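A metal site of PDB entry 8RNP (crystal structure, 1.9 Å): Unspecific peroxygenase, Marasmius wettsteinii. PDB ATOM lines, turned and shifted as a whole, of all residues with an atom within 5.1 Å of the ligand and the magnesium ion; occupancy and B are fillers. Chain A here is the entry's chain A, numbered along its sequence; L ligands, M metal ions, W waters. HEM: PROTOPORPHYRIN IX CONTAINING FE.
The side-chain carboxylate of Glu 89 is in hydrogen-bond range of the side-chain amide nitrogen of Asn 104, 3.0 Å away. A ring nitrogen (NE2) of His 90 lies within hydrogen-bond range of the side-chain carboxylate (OE1) of Glu 161. N of Leu 24 sits close to SG of Cys 21 (3.3 Å). The backbone NH (N) of Gly 23 lies close to the side-chain sulfur (SG) of Cys 21 (3.3 Å). OG of Ser 95 sits at hydrogen-bond distance from NH1 of Arg 96 (2.9 Å). OH of Tyr 53 is in hydrogen-bond range of O of Gly 23 (2.7 Å).
Water W4 lies within hydrogen-bond range of an oxygen (O1D) of the ligand and the side-chain carboxylate (OE1) of Glu 161. Water W3 lies within hydrogen-bond range of the backbone carbonyl oxygen of Pro 20 (2.7 Å) and an oxygen (O2A) of the ligand (2.8 Å).
Pro 20 touches the ligand. Pro 22 touches the ligand. Gly 23 touches the ligand (CA to C3C, 3.7 Å). Leu 24 touches the ligand (CD1 to C2B, 3.7 Å). Ile 45 touches the ligand (CG2 to CBB, 3.8 Å). CD2 of Tyr 53 touches CMC of the ligand (3.96 Å). Leu 60 touches the ligand (CD2 to CBB, 3.1 Å). O of Ala 63 touches CMB of the ligand (3.7 Å). Leu 82 touches the ligand. CG2 of Ile 88 touches CMA of the ligand, 3.4 Å away. Arg 96 touches the ligand (N to O2D, 3.8 Å). Glu 161 touches the ligand (OE2 to CHA, 3.3 Å). Phe 164 touches the ligand. Val 168 touches the ligand. Phe 187 touches the ligand (CZ to CBC, 3.4 Å). CZ of Phe 188 touches CMD of the ligand, at 3.9 Å. Hydrophobic or aromatic side chains that line the ligand: Pro 20, Pro 22, Leu 24, Ile 45, Tyr 53, Leu 60, Ala 63, Leu 82, Ile 88, His 90, Leu 94, Phe 164, Val 168, Phe 187 and Phe 188. 22 residues have an atom within 4 Å of the ligand: Pro 20, Cys 21, Pro 22, Gly 23, Leu 24, Ile 45, Tyr 53, Leu 60, Ala 63, Leu 82, Ile 88, Glu 89, His 90, Ser 93, Leu 94, Ser 95, Arg 96, Glu 161, Phe 164, Val 168, Phe 187 and Phe 188.
N of His 90 lies close to O1A of the ligand, at 2.9 Å. O2A of the ligand sits close to NE2 of His 90 (3.4 Å). FE of the ligand is bound by SG of Cys 21, at 2.3 Å. O1D of the ligand is in hydrogen-bond range of N of Leu 94 (2.6 Å). The backbone NH (N) of Ser 95 lies within hydrogen-bond range of an oxygen (O2D) of the ligand, 2.7 Å away. The side-chain hydroxyl (OG) of Ser 95 lies within hydrogen-bond range of an oxygen (O2D) of the ligand (2.6 Å).
Three residues have an atom within 4 Å of the magnesium ion: Glu 89, His 90 and Ser 93. The nearest printed residue that does not touch the magnesium ion is Asp 91 (4.4 Å).
The magnesium ion is bound by OE2 of Glu 89 (2.0 Å), O1A of the ligand (2.1 Å), OG of Ser 93 (2.1 Å), water W1 (2.1 Å), water W2 (2.2 Å) and O of His 90 (2.2 Å).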
ATOM      1  N   PRO A  20     -31.752   3.264  10.258  1.00  0.00           N
ATOM      2  CA  PRO A  20     -32.395   4.162  11.221  1.00  0.00           C
ATOM      3  C   PRO A  20     -32.070   5.645  11.011  1.00  0.00           C
ATOM      4  O   PRO A  20     -32.571   6.481  11.771  1.00  0.00           O
ATOM      5  CB  PRO A  20     -31.806   3.642  12.527  1.00  0.00           C
ATOM      6  CG  PRO A  20     -30.372   3.307  12.157  1.00  0.00           C
ATOM      7  CD  PRO A  20     -30.442   2.809  10.725  1.00  0.00           C
ATOM      8  N   CYS A  21     -31.272   5.942   9.985  1.00  0.00           N
ATOM      9  CA  CYS A  21     -30.862   7.299   9.629  1.00  0.00           C
ATOM     10  C   CYS A  21     -31.685   7.870   8.462  1.00  0.00           C
ATOM     11  O   CYS A  21     -31.532   7.441   7.319  1.00  0.00           O
ATOM     12  CB  CYS A  21     -29.417   7.346   9.155  1.00  0.00           C
ATOM     13  SG  CYS A  21     -28.891   9.025   8.728  1.00  0.00           S
ATOM     14  N   PRO A  22     -32.576   8.849   8.705  1.00  0.00           N
ATOM     15  CA  PRO A  22     -33.299   9.516   7.621  1.00  0.00           C
ATOM     16  C   PRO A  22     -32.394  10.214   6.607  1.00  0.00           C
ATOM     17  O   PRO A  22     -32.755  10.309   5.441  1.00  0.00           O
ATOM     18  CB  PRO A  22     -34.209  10.518   8.344  1.00  0.00           C
ATOM     19  CG  PRO A  22     -33.522  10.767   9.675  1.00  0.00           C
ATOM     20  CD  PRO A  22     -32.887   9.425  10.022  1.00  0.00           C
ATOM     21  N   GLY A  23     -31.236  10.721   7.062  1.00  0.00           N
ATOM     22  CA  GLY A  23     -30.284  11.407   6.202  1.00  0.00           C
ATOM     23  C   GLY A  23     -29.772  10.516   5.073  1.00  0.00           C
ATOM     24  O   GLY A  23     -29.788  10.903   3.896  1.00  0.00           O
ATOM     25  N   LEU A  24     -29.332   9.307   5.437  1.00  0.00           N
ATOM     26  CA  LEU A  24     -28.792   8.345   4.490  1.00  0.00           C
ATOM     27  C   LEU A  24     -29.928   7.690   3.694  1.00  0.00           C
ATOM     28  O   LEU A  24     -29.768   7.479   2.502  1.00  0.00           O
ATOM     29  CB  LEU A  24     -27.946   7.297   5.206  1.00  0.00           C
ATOM     30  CG  LEU A  24     -26.667   7.822   5.873  1.00  0.00           C
ATOM     31  CD1 LEU A  24     -25.871   6.644   6.452  1.00  0.00           C
ATOM     32  CD2 LEU A  24     -25.790   8.631   4.941  1.00  0.00           C
ATOM     33  N   ILE A  45     -20.570   7.774   0.815  1.00  0.00           N
ATOM     34  CA  ILE A  45     -21.327   8.594   1.742  1.00  0.00           C
ATOM     35  C   ILE A  45     -20.867  10.057   1.644  1.00  0.00           C
ATOM     36  O   ILE A  45     -21.683  10.971   1.648  1.00  0.00           O
ATOM     37  CB  ILE A  45     -21.215   8.060   3.191  1.00  0.00           C
ATOM     38  CG1 ILE A  45     -21.933   6.715   3.349  1.00  0.00           C
ATOM     39  CG2 ILE A  45     -21.754   9.098   4.178  1.00  0.00           C
ATOM     40  CD1 ILE A  45     -21.753   6.041   4.695  1.00  0.00           C
ATOM     41  N   TYR A  53     -26.692  17.435   0.126  1.00  0.00           N
ATOM     42  CA  TYR A  53     -26.982  18.279   1.274  1.00  0.00           C
ATOM     43  C   TYR A  53     -25.956  19.400   1.508  1.00  0.00           C
ATOM     44  O   TYR A  53     -26.228  20.296   2.297  1.00  0.00           O
ATOM     45  CB  TYR A  53     -26.985  17.459   2.571  1.00  0.00           C
ATOM     46  CG  TYR A  53     -27.997  16.327   2.662  1.00  0.00           C
ATOM     47  CD1 TYR A  53     -29.290  16.477   2.188  1.00  0.00           C
ATOM     48  CD2 TYR A  53     -27.656  15.137   3.297  1.00  0.00           C
ATOM     49  CE1 TYR A  53     -30.210  15.434   2.300  1.00  0.00           C
ATOM     50  CE2 TYR A  53     -28.561  14.088   3.394  1.00  0.00           C
ATOM     51  CZ  TYR A  53     -29.845  14.245   2.898  1.00  0.00           C
ATOM     52  OH  TYR A  53     -30.725  13.228   3.036  1.00  0.00           O
ATOM     53  N   VAL A  55     -23.160  18.743   2.957  1.00  0.00           N
ATOM     54  CA  VAL A  55     -22.467  18.331   4.170  1.00  0.00           C
ATOM     55  C   VAL A  55     -21.059  17.899   3.743  1.00  0.00           C
ATOM     56  O   VAL A  55     -20.909  17.083   2.824  1.00  0.00           O
ATOM     57  CB  VAL A  55     -23.217  17.202   4.894  1.00  0.00           C
ATOM     58  CG1 VAL A  55     -22.430  16.680   6.095  1.00  0.00           C
ATOM     59  CG2 VAL A  55     -24.604  17.646   5.339  1.00  0.00           C
ATOM     60  N   ILE A  59     -17.286  15.696   8.839  1.00  0.00           N
ATOM     61  CA  ILE A  59     -18.199  14.992   9.709  1.00  0.00           C
ATOM     62  C   ILE A  59     -18.584  13.636   9.103  1.00  0.00           C
ATOM     63  O   ILE A  59     -18.843  12.699   9.856  1.00  0.00           O
ATOM     64  CB  ILE A  59     -19.420  15.868  10.033  1.00  0.00           C
ATOM     65  CG1 ILE A  59     -20.302  15.148  11.049  1.00  0.00           C
ATOM     66  CG2 ILE A  59     -20.178  16.267   8.771  1.00  0.00           C
ATOM     67  CD1 ILE A  59     -21.271  16.067  11.776  1.00  0.00           C
ATOM     68  N   LEU A  60     -18.615  13.537   7.770  1.00  0.00           N
ATOM     69  CA  LEU A  60     -19.057  12.319   7.100  1.00  0.00           C
ATOM     70  C   LEU A  60     -17.986  11.241   7.187  1.00  0.00           C
ATOM     71  O   LEU A  60     -18.316  10.060   7.248  1.00  0.00           O
ATOM     72  CB  LEU A  60     -19.459  12.590   5.653  1.00  0.00           C
ATOM     73  CG  LEU A  60     -20.680  13.484   5.485  1.00  0.00           C
ATOM     74  CD1 LEU A  60     -21.037  13.713   4.023  1.00  0.00           C
ATOM     75  CD2 LEU A  60     -21.877  12.923   6.237  1.00  0.00           C
ATOM     76  N   ALA A  63     -18.199  10.128  11.184  1.00  0.00           N
ATOM     77  CA  ALA A  63     -19.371   9.299  11.385  1.00  0.00           C
ATOM     78  C   ALA A  63     -19.363   8.053  10.500  1.00  0.00           C
ATOM     79  O   ALA A  63     -19.766   6.966  10.928  1.00  0.00           O
ATOM     80  CB  ALA A  63     -20.610  10.126  11.100  1.00  0.00           C
ATOM     81  N   GLY A  64     -18.940   8.239   9.235  1.00  0.00           N
ATOM     82  CA  GLY A  64     -18.941   7.141   8.276  1.00  0.00           C
ATOM     83  C   GLY A  64     -18.122   5.943   8.765  1.00  0.00           C
ATOM     84  O   GLY A  64     -18.542   4.795   8.643  1.00  0.00           O
ATOM     85  N   GLY A  67     -19.738   4.138  11.495  1.00  0.00           N
ATOM     86  CA  GLY A  67     -20.800   3.336  10.924  1.00  0.00           C
ATOM     87  C   GLY A  67     -20.322   2.047  10.262  1.00  0.00           C
ATOM     88  O   GLY A  67     -21.048   1.049  10.265  1.00  0.00           O
ATOM     89  N   LEU A  82     -26.791  -0.282  10.146  1.00  0.00           N
ATOM     90  CA  LEU A  82     -26.576   0.839  11.061  1.00  0.00           C
ATOM     91  C   LEU A  82     -27.501   0.752  12.271  1.00  0.00           C
ATOM     92  O   LEU A  82     -27.365   1.546  13.197  1.00  0.00           O
ATOM     93  CB  LEU A  82     -26.767   2.170  10.327  1.00  0.00           C
ATOM     94  CG  LEU A  82     -25.692   2.526   9.300  1.00  0.00           C
ATOM     95  CD1 LEU A  82     -26.099   3.770   8.542  1.00  0.00           C
ATOM     96  CD2 LEU A  82     -24.343   2.722   9.987  1.00  0.00           C
ATOM     97  N   ILE A  88     -23.661   3.481  16.742  1.00  0.00           N
ATOM     98  CA  ILE A  88     -24.235   4.814  16.678  1.00  0.00           C
ATOM     99  C   ILE A  88     -25.665   4.782  17.181  1.00  0.00           C
ATOM    100  O   ILE A  88     -26.051   5.653  17.972  1.00  0.00           O
ATOM    101  CB  ILE A  88     -24.114   5.416  15.269  1.00  0.00           C
ATOM    102  CG1 ILE A  88     -22.648   5.650  14.895  1.00  0.00           C
ATOM    103  CG2 ILE A  88     -24.916   6.711  15.138  1.00  0.00           C
ATOM    104  CD1 ILE A  88     -22.448   5.941  13.422  1.00  0.00           C
ATOM    105  N   GLU A  89     -26.448   3.783  16.764  1.00  0.00           N
ATOM    106  CA  GLU A  89     -27.865   3.736  17.128  1.00  0.00           C
ATOM    107  C   GLU A  89     -27.992   3.773  18.653  1.00  0.00           C
ATOM    108  O   GLU A  89     -27.216   3.164  19.373  1.00  0.00           O
ATOM    109  CB  GLU A  89     -28.532   2.522  16.497  1.00  0.00           C
ATOM    110  CG  GLU A  89     -30.057   2.561  16.565  1.00  0.00           C
ATOM    111  CD  GLU A  89     -30.678   2.267  17.912  1.00  0.00           C
ATOM    112  OE1 GLU A  89     -30.184   1.315  18.541  1.00  0.00           O
ATOM    113  OE2 GLU A  89     -31.690   2.925  18.289  1.00  0.00           O
ATOM    114  N   HIS A  90     -29.011   4.488  19.121  1.00  0.00           N
ATOM    115  CA  HIS A  90     -29.147   4.829  20.517  1.00  0.00           C
ATOM    116  C   HIS A  90     -30.616   4.960  20.893  1.00  0.00           C
ATOM    117  O   HIS A  90     -31.468   5.209  20.035  1.00  0.00           O
ATOM    118  CB  HIS A  90     -28.435   6.171  20.762  1.00  0.00           C
ATOM    119  CG  HIS A  90     -28.945   7.276  19.897  1.00  0.00           C
ATOM    120  ND1 HIS A  90     -30.197   7.816  20.087  1.00  0.00           N
ATOM    121  CD2 HIS A  90     -28.419   7.897  18.824  1.00  0.00           C
ATOM    122  CE1 HIS A  90     -30.398   8.780  19.180  1.00  0.00           C
ATOM    123  NE2 HIS A  90     -29.329   8.850  18.410  1.00  0.00           N
ATOM    124  N   ASP A  91     -30.878   4.853  22.204  1.00  0.00           N
ATOM    125  CA  ASP A  91     -32.192   5.108  22.776  1.00  0.00           C
ATOM    126  C   ASP A  91     -32.559   6.577  22.621  1.00  0.00           C
ATOM    127  O   ASP A  91     -31.690   7.425  22.395  1.00  0.00           O
ATOM    128  CB  ASP A  91     -32.203   4.663  24.241  1.00  0.00           C
ATOM    129  CG  ASP A  91     -32.035   3.163  24.466  1.00  0.00           C
ATOM    130  OD1 ASP A  91     -32.377   2.386  23.546  1.00  0.00           O
ATOM    131  OD2 ASP A  91     -31.505   2.772  25.542  1.00  0.00           O
ATOM    132  N   SER A  93     -34.394   8.081  20.360  1.00  0.00           N
ATOM    133  CA  SER A  93     -34.432   8.557  18.991  1.00  0.00           C
ATOM    134  C   SER A  93     -35.645   9.470  18.782  1.00  0.00           C
ATOM    135  O   SER A  93     -36.609   9.419  19.531  1.00  0.00           O
ATOM    136  CB  SER A  93     -34.458   7.394  18.051  1.00  0.00           C
ATOM    137  OG  SER A  93     -33.194   6.758  17.982  1.00  0.00           O
ATOM    138  N   LEU A  94     -35.580  10.302  17.740  1.00  0.00           N
ATOM    139  CA  LEU A  94     -36.630  11.253  17.397  1.00  0.00           C
ATOM    140  C   LEU A  94     -37.813  10.584  16.703  1.00  0.00           C
ATOM    141  O   LEU A  94     -38.916  11.124  16.777  1.00  0.00           O
ATOM    142  CB  LEU A  94     -36.048  12.340  16.499  1.00  0.00           C
ATOM    143  CG  LEU A  94     -34.925  13.181  17.102  1.00  0.00           C
ATOM    144  CD1 LEU A  94     -34.184  13.933  16.018  1.00  0.00           C
ATOM    145  CD2 LEU A  94     -35.516  14.131  18.131  1.00  0.00           C
ATOM    146  N   SER A  95     -37.569   9.481  15.989  1.00  0.00           N
ATOM    147  CA  SER A  95     -38.562   8.937  15.072  1.00  0.00           C
ATOM    148  C   SER A  95     -38.599   7.412  15.122  1.00  0.00           C
ATOM    149  O   SER A  95     -39.396   6.809  14.403  1.00  0.00           O
ATOM    150  CB  SER A  95     -38.320   9.418  13.643  1.00  0.00           C
ATOM    151  OG  SER A  95     -37.112   8.915  13.096  1.00  0.00           O
ATOM    152  N   ARG A  96     -37.734   6.794  15.935  1.00  0.00           N
ATOM    153  CA  ARG A  96     -37.715   5.341  16.115  1.00  0.00           C
ATOM    154  C   ARG A  96     -37.926   5.021  17.597  1.00  0.00           C
ATOM    155  O   ARG A  96     -37.755   5.888  18.441  1.00  0.00           O
ATOM    156  CB  ARG A  96     -36.377   4.743  15.664  1.00  0.00           C
ATOM    157  CG  ARG A  96     -36.273   4.385  14.180  1.00  0.00           C
ATOM    158  CD  ARG A  96     -36.364   5.586  13.234  1.00  0.00           C
ATOM    159  NE  ARG A  96     -35.986   5.210  11.874  1.00  0.00           N
ATOM    160  CZ  ARG A  96     -36.162   5.945  10.771  1.00  0.00           C
ATOM    161  NH1 ARG A  96     -36.636   7.175  10.838  1.00  0.00           N
ATOM    162  NH2 ARG A  96     -35.863   5.439   9.587  1.00  0.00           N
ATOM    163  N   GLU A  97     -38.256   3.760  17.875  1.00  0.00           N
ATOM    164  CA  GLU A  97     -38.419   3.265  19.244  1.00  0.00           C
ATOM    165  C   GLU A  97     -37.107   2.688  19.758  1.00  0.00           C
ATOM    166  O   GLU A  97     -36.258   2.253  18.979  1.00  0.00           O
ATOM    167  CB  GLU A  97     -39.455   2.134  19.330  1.00  0.00           C
ATOM    168  CG  GLU A  97     -40.801   2.486  18.695  1.00  0.00           C
ATOM    169  CD  GLU A  97     -41.814   1.357  18.653  1.00  0.00           C
ATOM    170  OE1 GLU A  97     -41.459   0.242  18.243  1.00  0.00           O
ATOM    171  OE2 GLU A  97     -42.990   1.640  18.972  1.00  0.00           O
ATOM    172  N   ASN A 104     -36.248  -0.346  16.405  1.00  0.00           N
ATOM    173  CA  ASN A 104     -35.270   0.734  16.439  1.00  0.00           C
ATOM    174  C   ASN A 104     -34.828   1.122  15.028  1.00  0.00           C
ATOM    175  O   ASN A 104     -33.889   1.903  14.882  1.00  0.00           O
ATOM    176  CB  ASN A 104     -34.041   0.399  17.287  1.00  0.00           C
ATOM    177  CG  ASN A 104     -33.125  -0.619  16.653  1.00  0.00           C
ATOM    178  OD1 ASN A 104     -33.544  -1.405  15.800  1.00  0.00           O
ATOM    179  ND2 ASN A 104     -31.872  -0.618  17.060  1.00  0.00           N
ATOM    180  N   GLU A 161     -27.643  14.916  15.614  1.00  0.00           N
ATOM    181  CA  GLU A 161     -28.702  14.535  14.720  1.00  0.00           C
ATOM    182  C   GLU A 161     -29.725  15.667  14.638  1.00  0.00           C
ATOM    183  O   GLU A 161     -30.191  15.963  13.538  1.00  0.00           O
ATOM    184  CB  GLU A 161     -29.248  13.162  15.145  1.00  0.00           C
ATOM    185  CG  GLU A 161     -28.183  12.080  14.966  1.00  0.00           C
ATOM    186  CD  GLU A 161     -28.364  10.766  15.720  1.00  0.00           C
ATOM    187  OE1 GLU A 161     -29.238  10.682  16.611  1.00  0.00           O
ATOM    188  OE2 GLU A 161     -27.643   9.812  15.352  1.00  0.00           O
ATOM    189  N   PHE A 164     -28.393  18.254  12.512  1.00  0.00           N
ATOM    190  CA  PHE A 164     -28.515  17.867  11.115  1.00  0.00           C
ATOM    191  C   PHE A 164     -29.875  18.270  10.550  1.00  0.00           C
ATOM    192  O   PHE A 164     -29.952  18.892   9.505  1.00  0.00           O
ATOM    193  CB  PHE A 164     -28.284  16.377  10.926  1.00  0.00           C
ATOM    194  CG  PHE A 164     -26.884  15.969  10.555  1.00  0.00           C
ATOM    195  CD1 PHE A 164     -26.148  16.711   9.635  1.00  0.00           C
ATOM    196  CD2 PHE A 164     -26.337  14.808  11.066  1.00  0.00           C
ATOM    197  CE1 PHE A 164     -24.872  16.306   9.260  1.00  0.00           C
ATOM    198  CE2 PHE A 164     -25.051  14.419  10.701  1.00  0.00           C
ATOM    199  CZ  PHE A 164     -24.336  15.161   9.785  1.00  0.00           C
ATOM    200  N   TYR A 165     -30.981  17.899  11.191  1.00  0.00           N
ATOM    201  CA  TYR A 165     -32.265  18.212  10.600  1.00  0.00           C
ATOM    202  C   TYR A 165     -32.459  19.722  10.515  1.00  0.00           C
ATOM    203  O   TYR A 165     -33.037  20.200   9.532  1.00  0.00           O
ATOM    204  CB  TYR A 165     -33.403  17.416  11.251  1.00  0.00           C
ATOM    205  CG  TYR A 165     -33.989  17.910  12.567  1.00  0.00           C
ATOM    206  CD1 TYR A 165     -34.788  19.047  12.633  1.00  0.00           C
ATOM    207  CD2 TYR A 165     -33.850  17.158  13.728  1.00  0.00           C
ATOM    208  CE1 TYR A 165     -35.332  19.479  13.830  1.00  0.00           C
ATOM    209  CE2 TYR A 165     -34.403  17.572  14.925  1.00  0.00           C
ATOM    210  CZ  TYR A 165     -35.149  18.729  14.982  1.00  0.00           C
ATOM    211  OH  TYR A 165     -35.721  19.096  16.188  1.00  0.00           O
ATOM    212  N   VAL A 168     -29.656  20.865   7.472  1.00  0.00           N
ATOM    213  CA  VAL A 168     -29.722  20.319   6.137  1.00  0.00           C
ATOM    214  C   VAL A 168     -31.060  20.668   5.490  1.00  0.00           C
ATOM    215  O   VAL A 168     -31.119  20.899   4.293  1.00  0.00           O
ATOM    216  CB  VAL A 168     -29.453  18.797   6.184  1.00  0.00           C
ATOM    217  CG1 VAL A 168     -29.902  18.085   4.923  1.00  0.00           C
ATOM    218  CG2 VAL A 168     -27.976  18.499   6.457  1.00  0.00           C
ATOM    219  N   PHE A 187     -38.956  15.132   5.381  1.00  0.00           N
ATOM    220  CA  PHE A 187     -37.681  14.466   5.532  1.00  0.00           C
ATOM    221  C   PHE A 187     -37.848  13.199   6.382  1.00  0.00           C
ATOM    222  O   PHE A 187     -37.328  12.139   6.035  1.00  0.00           O
ATOM    223  CB  PHE A 187     -36.701  15.471   6.124  1.00  0.00           C
ATOM    224  CG  PHE A 187     -35.302  14.945   6.409  1.00  0.00           C
ATOM    225  CD1 PHE A 187     -34.433  14.659   5.374  1.00  0.00           C
ATOM    226  CD2 PHE A 187     -34.834  14.811   7.702  1.00  0.00           C
ATOM    227  CE1 PHE A 187     -33.146  14.185   5.617  1.00  0.00           C
ATOM    228  CE2 PHE A 187     -33.561  14.332   7.948  1.00  0.00           C
ATOM    229  CZ  PHE A 187     -32.711  14.032   6.905  1.00  0.00           C
ATOM    230  N   PHE A 188     -38.603  13.300   7.484  1.00  0.00           N
ATOM    231  CA  PHE A 188     -38.703  12.188   8.409  1.00  0.00           C
ATOM    232  C   PHE A 188     -39.759  11.194   7.938  1.00  0.00           C
ATOM    233  O   PHE A 188     -39.549   9.985   7.992  1.00  0.00           O
ATOM    234  CB  PHE A 188     -39.044  12.700   9.808  1.00  0.00           C
ATOM    235  CG  PHE A 188     -37.838  13.080  10.660  1.00  0.00           C
ATOM    236  CD1 PHE A 188     -37.181  12.118  11.407  1.00  0.00           C
ATOM    237  CD2 PHE A 188     -37.389  14.392  10.733  1.00  0.00           C
ATOM    238  CE1 PHE A 188     -36.105  12.459  12.221  1.00  0.00           C
ATOM    239  CE2 PHE A 188     -36.299  14.727  11.522  1.00  0.00           C
ATOM    240  CZ  PHE A 188     -35.658  13.761  12.262  1.00  0.00           C
HETATM  241  CHA HEM L   1     -29.777   9.033  12.947  1.00  0.00           C
HETATM  242  CHB HEM L   1     -25.872   7.043  11.069  1.00  0.00           C
HETATM  243  CHC HEM L   1     -25.272  10.967   8.245  1.00  0.00           C
HETATM  244  CHD HEM L   1     -29.358  12.800   9.970  1.00  0.00           C
HETATM  245  C1A HEM L   1     -28.783   8.161  12.652  1.00  0.00           C
HETATM  246  C2A HEM L   1     -28.656   6.895  13.253  1.00  0.00           C
HETATM  247  C3A HEM L   1     -27.548   6.337  12.722  1.00  0.00           C
HETATM  248  C4A HEM L   1     -27.010   7.258  11.814  1.00  0.00           C
HETATM  249  CMA HEM L   1     -26.984   4.973  13.010  1.00  0.00           C
HETATM  250  CAA HEM L   1     -29.571   6.245  14.274  1.00  0.00           C
HETATM  251  CBA HEM L   1     -29.401   6.973  15.606  1.00  0.00           C
HETATM  252  CGA HEM L   1     -30.651   6.777  16.422  1.00  0.00           C
HETATM  253  O1A HEM L   1     -30.758   5.824  17.263  1.00  0.00           O
HETATM  254  O2A HEM L   1     -31.617   7.565  16.248  1.00  0.00           O
HETATM  255  C1B HEM L   1     -25.365   7.989  10.171  1.00  0.00           C
HETATM  256  C2B HEM L   1     -24.150   7.780   9.491  1.00  0.00           C
HETATM  257  C3B HEM L   1     -23.956   8.848   8.696  1.00  0.00           C
HETATM  258  C4B HEM L   1     -25.110   9.760   8.916  1.00  0.00           C
HETATM  259  CMB HEM L   1     -23.162   6.643   9.539  1.00  0.00           C
HETATM  260  CAB HEM L   1     -22.729   8.999   7.911  1.00  0.00           C
HETATM  261  CBB HEM L   1     -22.207  10.192   7.748  1.00  0.00           C
HETATM  262  C1C HEM L   1     -26.364  11.798   8.371  1.00  0.00           C
HETATM  263  C2C HEM L   1     -26.628  12.910   7.566  1.00  0.00           C
HETATM  264  C3C HEM L   1     -27.801  13.442   8.067  1.00  0.00           C
HETATM  265  C4C HEM L   1     -28.247  12.630   9.173  1.00  0.00           C
HETATM  266  CMC HEM L   1     -25.835  13.420   6.371  1.00  0.00           C
HETATM  267  CAC HEM L   1     -28.406  14.599   7.434  1.00  0.00           C
HETATM  268  CBC HEM L   1     -29.578  15.123   7.739  1.00  0.00           C
HETATM  269  C1D HEM L   1     -29.762  11.904  10.954  1.00  0.00           C
HETATM  270  C2D HEM L   1     -30.908  12.210  11.856  1.00  0.00           C
HETATM  271  C3D HEM L   1     -31.031  11.132  12.676  1.00  0.00           C
HETATM  272  C4D HEM L   1     -29.924  10.232  12.302  1.00  0.00           C
HETATM  273  CMD HEM L   1     -31.821  13.433  11.854  1.00  0.00           C
HETATM  274  CAD HEM L   1     -32.055  11.026  13.803  1.00  0.00           C
HETATM  275  CBD HEM L   1     -32.962   9.781  13.807  1.00  0.00           C
HETATM  276  CGD HEM L   1     -33.984   9.806  14.927  1.00  0.00           C
HETATM  277  O1D HEM L   1     -33.668  10.284  16.046  1.00  0.00           O
HETATM  278  O2D HEM L   1     -35.120   9.284  14.785  1.00  0.00           O
HETATM  279  NA  HEM L   1     -27.787   8.377  11.740  1.00  0.00           N
HETATM  280  NB  HEM L   1     -25.912   9.159   9.815  1.00  0.00           N
HETATM  281  NC  HEM L   1     -27.342  11.640   9.296  1.00  0.00           N
HETATM  282  ND  HEM L   1     -29.223  10.706  11.246  1.00  0.00           N
HETATM  283 FE   HEM L   1     -27.724   9.939  10.463  1.00  0.00          FE
HETATM  284 MG    MG M   1     -32.382   4.821  18.058  1.00  0.00          MG
HETATM  285  O   HOH W   1     -33.172   4.231  16.165  1.00  0.00           O
HETATM  286  O   HOH W   2     -34.200   4.234  19.066  1.00  0.00           O
HETATM  287  O   HOH W   3     -33.365   6.403  14.375  1.00  0.00           O
HETATM  288  O   HOH W   4     -31.703  11.329  17.581  1.00  0.00           O
